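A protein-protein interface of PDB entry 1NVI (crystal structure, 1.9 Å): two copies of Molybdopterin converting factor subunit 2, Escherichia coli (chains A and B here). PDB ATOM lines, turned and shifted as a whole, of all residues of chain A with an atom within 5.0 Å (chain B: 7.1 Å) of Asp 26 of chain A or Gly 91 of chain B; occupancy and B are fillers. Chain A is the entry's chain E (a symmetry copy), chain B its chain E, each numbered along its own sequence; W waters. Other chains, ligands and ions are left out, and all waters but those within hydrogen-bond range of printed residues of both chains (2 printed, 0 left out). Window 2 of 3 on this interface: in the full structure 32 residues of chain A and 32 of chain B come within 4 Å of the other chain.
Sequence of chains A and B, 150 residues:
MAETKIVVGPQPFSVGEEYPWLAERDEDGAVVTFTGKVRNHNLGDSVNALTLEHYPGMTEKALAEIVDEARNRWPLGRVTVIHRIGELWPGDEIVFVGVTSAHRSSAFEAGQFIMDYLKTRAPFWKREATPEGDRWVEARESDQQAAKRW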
ATOM      1  N   GLU A  24      18.938  -7.697 -16.080  1.00  0.00           N
ATOM      2  CA  GLU A  24      19.130  -9.104 -15.692  1.00  0.00           C
ATOM      3  C   GLU A  24      19.921  -9.935 -16.703  1.00  0.00           C
ATOM      4  O   GLU A  24      20.795 -10.722 -16.320  1.00  0.00           O
ATOM      5  CB  GLU A  24      17.767  -9.793 -15.470  1.00  0.00           C
ATOM      6  CG  GLU A  24      17.560 -10.419 -14.093  1.00  0.00           C
ATOM      7  CD  GLU A  24      16.077 -10.589 -13.741  1.00  0.00           C
ATOM      8  OE1 GLU A  24      15.374 -11.315 -14.467  1.00  0.00           O
ATOM      9  OE2 GLU A  24      15.595  -9.988 -12.748  1.00  0.00           O
ATOM     10  N   ARG A  25      19.597  -9.778 -17.987  1.00  0.00           N
ATOM     11  CA  ARG A  25      20.168 -10.623 -19.045  1.00  0.00           C
ATOM     12  C   ARG A  25      21.597 -10.229 -19.413  1.00  0.00           C
ATOM     13  O   ARG A  25      21.857  -9.075 -19.790  1.00  0.00           O
ATOM     14  CB  ARG A  25      19.285 -10.564 -20.289  1.00  0.00           C
ATOM     15  CG  ARG A  25      17.832 -11.019 -20.047  1.00  0.00           C
ATOM     16  CD  ARG A  25      17.064 -11.421 -21.325  1.00  0.00           C
ATOM     17  NE  ARG A  25      17.377 -10.553 -22.471  1.00  0.00           N
ATOM     18  CZ  ARG A  25      16.994 -10.790 -23.730  1.00  0.00           C
ATOM     19  NH1 ARG A  25      16.258 -11.855 -24.035  1.00  0.00           N
ATOM     20  NH2 ARG A  25      17.350  -9.954 -24.697  1.00  0.00           N
ATOM     21  N   ASP A  26      22.507 -11.190 -19.311  1.00  0.00           N
ATOM     22  CA  ASP A  26      23.922 -10.982 -19.611  1.00  0.00           C
ATOM     23  C   ASP A  26      24.160 -10.670 -21.087  1.00  0.00           C
ATOM     24  O   ASP A  26      25.164 -10.051 -21.432  1.00  0.00           O
ATOM     25  CB  ASP A  26      24.757 -12.228 -19.243  1.00  0.00           C
ATOM     26  CG  ASP A  26      24.979 -12.396 -17.731  1.00  0.00           C
ATOM     27  OD1 ASP A  26      24.624 -11.505 -16.937  1.00  0.00           O
ATOM     28  OD2 ASP A  26      25.519 -13.416 -17.245  1.00  0.00           O
ATOM     29  N   GLU A  27      23.257 -11.099 -21.963  1.00  0.00           N
ATOM     30  CA  GLU A  27      23.459 -10.918 -23.399  1.00  0.00           C
ATOM     31  C   GLU A  27      23.234  -9.468 -23.819  1.00  0.00           C
ATOM     32  O   GLU A  27      23.716  -9.043 -24.860  1.00  0.00           O
ATOM     33  CB  GLU A  27      22.568 -11.862 -24.217  1.00  0.00           C
ATOM     34  CG  GLU A  27      21.073 -11.703 -23.988  1.00  0.00           C
ATOM     35  CD  GLU A  27      20.491 -12.828 -23.155  1.00  0.00           C
ATOM     36  OE1 GLU A  27      21.091 -13.175 -22.098  1.00  0.00           O
ATOM     37  OE2 GLU A  27      19.435 -13.369 -23.559  1.00  0.00           O
ATOM     38  N   ASP A  28      22.489  -8.723 -23.018  1.00  0.00           N
ATOM     39  CA  ASP A  28      22.279  -7.304 -23.250  1.00  0.00           C
ATOM     40  C   ASP A  28      23.388  -6.491 -22.585  1.00  0.00           C
ATOM     41  O   ASP A  28      23.292  -6.150 -21.400  1.00  0.00           O
ATOM     42  CB  ASP A  28      20.955  -6.862 -22.660  1.00  0.00           C
ATOM     43  CG  ASP A  28      19.772  -7.582 -23.257  1.00  0.00           C
ATOM     44  OD1 ASP A  28      19.782  -7.860 -24.480  1.00  0.00           O
ATOM     45  OD2 ASP A  28      18.772  -7.877 -22.562  1.00  0.00           O
ATOM     46  N   GLY A  29      24.424  -6.175 -23.346  1.00  0.00           N
ATOM     47  CA  GLY A  29      25.526  -5.362 -22.851  1.00  0.00           C
ATOM     48  C   GLY A  29      25.232  -3.893 -22.577  1.00  0.00           C
ATOM     49  O   GLY A  29      26.015  -3.253 -21.899  1.00  0.00           O
ATOM     50  N   GLY B  36      26.945   0.020 -19.215  1.00  0.00           N
ATOM     51  CA  GLY B  36      27.626  -0.918 -20.082  1.00  0.00           C
ATOM     52  C   GLY B  36      28.095  -2.091 -19.220  1.00  0.00           C
ATOM     53  O   GLY B  36      28.661  -1.890 -18.141  1.00  0.00           O
ATOM     54  N   LYS B  37      27.869  -3.303 -19.698  1.00  0.00           N
ATOM     55  CA  LYS B  37      28.206  -4.516 -18.963  1.00  0.00           C
ATOM     56  C   LYS B  37      29.118  -5.403 -19.796  1.00  0.00           C
ATOM     57  O   LYS B  37      29.117  -5.324 -21.024  1.00  0.00           O
ATOM     58  CB  LYS B  37      26.924  -5.302 -18.625  1.00  0.00           C
ATOM     59  CG  LYS B  37      25.727  -4.451 -18.224  1.00  0.00           C
ATOM     60  CD  LYS B  37      24.570  -5.270 -17.634  1.00  0.00           C
ATOM     61  CE  LYS B  37      24.345  -6.558 -18.388  1.00  0.00           C
ATOM     62  NZ  LYS B  37      22.959  -7.006 -18.281  1.00  0.00           N
ATOM     63  N   VAL B  38      29.892  -6.257 -19.134  1.00  0.00           N
ATOM     64  CA  VAL B  38      30.570  -7.372 -19.808  1.00  0.00           C
ATOM     65  C   VAL B  38      29.527  -8.407 -20.272  1.00  0.00           C
ATOM     66  O   VAL B  38      28.747  -8.913 -19.461  1.00  0.00           O
ATOM     67  CB  VAL B  38      31.584  -8.085 -18.863  1.00  0.00           C
ATOM     68  CG1 VAL B  38      32.428  -9.089 -19.631  1.00  0.00           C
ATOM     69  CG2 VAL B  38      32.484  -7.074 -18.143  1.00  0.00           C
ATOM     70  N   ARG B  39      29.499  -8.720 -21.567  1.00  0.00           N
ATOM     71  CA  ARG B  39      28.630  -9.791 -22.082  1.00  0.00           C
ATOM     72  C   ARG B  39      29.374 -11.135 -22.015  1.00  0.00           C
ATOM     73  O   ARG B  39      28.766 -12.183 -21.760  1.00  0.00           O
ATOM     74  CB  ARG B  39      28.172  -9.530 -23.530  1.00  0.00           C
ATOM     75  CG  ARG B  39      27.820  -8.079 -23.875  1.00  0.00           C
ATOM     76  CD  ARG B  39      27.724  -7.817 -25.373  1.00  0.00           C
ATOM     77  NE  ARG B  39      26.595  -8.537 -25.952  1.00  0.00           N
ATOM     78  CZ  ARG B  39      26.561  -9.082 -27.171  1.00  0.00           C
ATOM     79  NH1 ARG B  39      25.456  -9.712 -27.563  1.00  0.00           N
ATOM     80  NH2 ARG B  39      27.603  -9.009 -28.001  1.00  0.00           N
ATOM     81  N   LEU B  88      37.116  -8.250 -13.779  1.00  0.00           N
ATOM     82  CA  LEU B  88      35.670  -8.249 -13.889  1.00  0.00           C
ATOM     83  C   LEU B  88      35.258  -9.559 -14.531  1.00  0.00           C
ATOM     84  O   LEU B  88      36.091 -10.280 -15.072  1.00  0.00           O
ATOM     85  CB  LEU B  88      35.202  -7.067 -14.733  1.00  0.00           C
ATOM     86  CG  LEU B  88      35.601  -5.666 -14.267  1.00  0.00           C
ATOM     87  CD1 LEU B  88      35.147  -4.611 -15.295  1.00  0.00           C
ATOM     88  CD2 LEU B  88      34.985  -5.361 -12.893  1.00  0.00           C
ATOM     89  N   TRP B  89      33.983  -9.875 -14.437  1.00  0.00           N
ATOM     90  CA  TRP B  89      33.445 -11.145 -14.920  1.00  0.00           C
ATOM     91  C   TRP B  89      32.311 -10.848 -15.888  1.00  0.00           C
ATOM     92  O   TRP B  89      31.735  -9.764 -15.831  1.00  0.00           O
ATOM     93  CB  TRP B  89      32.930 -11.999 -13.748  1.00  0.00           C
ATOM     94  CG  TRP B  89      34.010 -12.368 -12.778  1.00  0.00           C
ATOM     95  CD1 TRP B  89      34.288 -11.759 -11.584  1.00  0.00           C
ATOM     96  CD2 TRP B  89      34.991 -13.393 -12.940  1.00  0.00           C
ATOM     97  NE1 TRP B  89      35.379 -12.347 -10.994  1.00  0.00           N
ATOM     98  CE2 TRP B  89      35.826 -13.362 -11.801  1.00  0.00           C
ATOM     99  CE3 TRP B  89      35.252 -14.345 -13.933  1.00  0.00           C
ATOM    100  CZ2 TRP B  89      36.890 -14.230 -11.634  1.00  0.00           C
ATOM    101  CZ3 TRP B  89      36.308 -15.211 -13.761  1.00  0.00           C
ATOM    102  CH2 TRP B  89      37.108 -15.160 -12.614  1.00  0.00           C
ATOM    103  N   PRO B  90      32.008 -11.786 -16.791  1.00  0.00           N
ATOM    104  CA  PRO B  90      30.788 -11.713 -17.603  1.00  0.00           C
ATOM    105  C   PRO B  90      29.569 -11.376 -16.770  1.00  0.00           C
ATOM    106  O   PRO B  90      29.301 -12.051 -15.781  1.00  0.00           O
ATOM    107  CB  PRO B  90      30.657 -13.138 -18.160  1.00  0.00           C
ATOM    108  CG  PRO B  90      32.050 -13.605 -18.289  1.00  0.00           C
ATOM    109  CD  PRO B  90      32.823 -12.965 -17.145  1.00  0.00           C
ATOM    110  N   GLY B  91      28.860 -10.327 -17.163  1.00  0.00           N
ATOM    111  CA  GLY B  91      27.647  -9.903 -16.493  1.00  0.00           C
ATOM    112  C   GLY B  91      27.879  -8.707 -15.586  1.00  0.00           C
ATOM    113  O   GLY B  91      26.923  -8.055 -15.172  1.00  0.00           O
ATOM    114  N   ASP B  92      29.142  -8.435 -15.258  1.00  0.00           N
ATOM    115  CA  ASP B  92      29.484  -7.308 -14.386  1.00  0.00           C
ATOM    116  C   ASP B  92      29.215  -6.015 -15.132  1.00  0.00           C
ATOM    117  O   ASP B  92      29.445  -5.935 -16.334  1.00  0.00           O
ATOM    118  CB  ASP B  92      30.955  -7.330 -13.980  1.00  0.00           C
ATOM    119  CG  ASP B  92      31.258  -8.333 -12.889  1.00  0.00           C
ATOM    120  OD1 ASP B  92      30.326  -8.917 -12.290  1.00  0.00           O
ATOM    121  OD2 ASP B  92      32.429  -8.588 -12.557  1.00  0.00           O
ATOM    122  N   GLU B  93      28.755  -5.007 -14.405  1.00  0.00           N
ATOM    123  CA  GLU B  93      28.546  -3.686 -14.954  1.00  0.00           C
ATOM    124  C   GLU B  93      29.893  -2.981 -14.870  1.00  0.00           C
ATOM    125  O   GLU B  93      30.531  -2.959 -13.820  1.00  0.00           O
ATOM    126  CB  GLU B  93      27.433  -2.962 -14.178  1.00  0.00           C
ATOM    127  CG  GLU B  93      26.156  -3.811 -14.152  1.00  0.00           C
ATOM    128  CD  GLU B  93      24.911  -3.115 -13.632  1.00  0.00           C
ATOM    129  OE1 GLU B  93      24.999  -2.264 -12.712  1.00  0.00           O
ATOM    130  OE2 GLU B  93      23.821  -3.463 -14.139  1.00  0.00           O
ATOM    131  N   ILE B  94      30.331  -2.434 -15.993  1.00  0.00           N
ATOM    132  CA  ILE B  94      31.671  -1.872 -16.107  1.00  0.00           C
ATOM    133  C   ILE B  94      31.644  -0.352 -16.098  1.00  0.00           C
ATOM    134  O   ILE B  94      32.551   0.260 -15.570  1.00  0.00           O
ATOM    135  CB  ILE B  94      32.475  -2.463 -17.350  1.00  0.00           C
ATOM    136  CG1 ILE B  94      33.476  -1.458 -17.921  1.00  0.00           C
ATOM    137  CG2 ILE B  94      31.599  -2.896 -18.471  1.00  0.00           C
ATOM    138  CD1 ILE B  94      34.154  -1.950 -19.195  1.00  0.00           C
HETATM  139  O   HOH W   1      23.858  -9.105 -16.543  1.00  0.00           O
HETATM  140  O   HOH W   2      20.350  -6.544 -19.533  1.00  0.00           O
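Asp 26 of chain A touches two residues of chain B. Of chain A, only Asp 26 comes within 4 Å of Gly 91 of chain B. Of the printed residues of chain B, Asp 28 of chain A touches Lys 37 (3.2 Å). Of the printed residues of chain B, Arg 25 of chain A touches Lys 37. The nearest residue of chain B that does not touch Asp 26 of chain A is Val 38 of chain B (4.2 Å). The nearest printed residue of chain A that does not touch Gly 91 of chain B is Arg 25 of chain A (6.7 Å).
NZ of Lys 37 of chain B lies close to O of Asp 28 of chain A (3.3 Å). The guanidinium group (NE) of Arg 39 of chain B lies within hydrogen-bond range of the backbone carbonyl oxygen (O) of Glu 27 of chain A. NZ of Lys 37 of chain B lies within hydrogen-bond range of O of Arg 25 of chain A, 2.8 Å away. The backbone carbonyl oxygen (O) of Gly 29 of chain A is in hydrogen-bond range of the backbone NH (N) of Lys 37 of chain B, at 2.9 Å.
No position is printed for both chains.
Water W1 lies within hydrogen-bond range of OD1 of Asp 26 of chain A (2.5 Å), NZ of Lys 37 of chain B (2.9 Å) and O of Glu 24 of chain A (3.5 Å). Water W2 bridges the side-chain amino group (NZ) of Lys 37 of chain B and the backbone carbonyl oxygen (O) of Arg 25 of chain A.
The guanidinium group (NE) of Arg 25 of chain A is in salt-bridge range of the side-chain carboxylate (OD2) of Asp 28 of chain A, 3.0 Å away. O of Gly 36 of chain B lies within hydrogen-bond range of N of Ile 94 of chain B, 2.8 Å away. The guanidinium group of Arg 25 of chain A is in salt-bridge range of the side-chain carboxylate of Glu 27 of chain A (3.6 Å). The backbone carbonyl oxygen of Val 38 of chain B lies within hydrogen-bond range of the backbone NH of Gly 91 of chain B (2.7 Å).
Asp 26 of chain A touches Arg 39 of chain B (O to CA, 3.5 Å). Asp 26 of chain A touches Gly 91 of chain B (OD1 to CA, 3.4 Å). Gly 29 of chain A touches Gly 36 of chain B (O to CA, 3.4 Å). Gly 29 of chain A touches Arg 39 of chain B.
Among the printed residues, no Asp or Glu carboxylate lies within 4 Å of a Lys or Arg side-chain nitrogen of the other chain.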
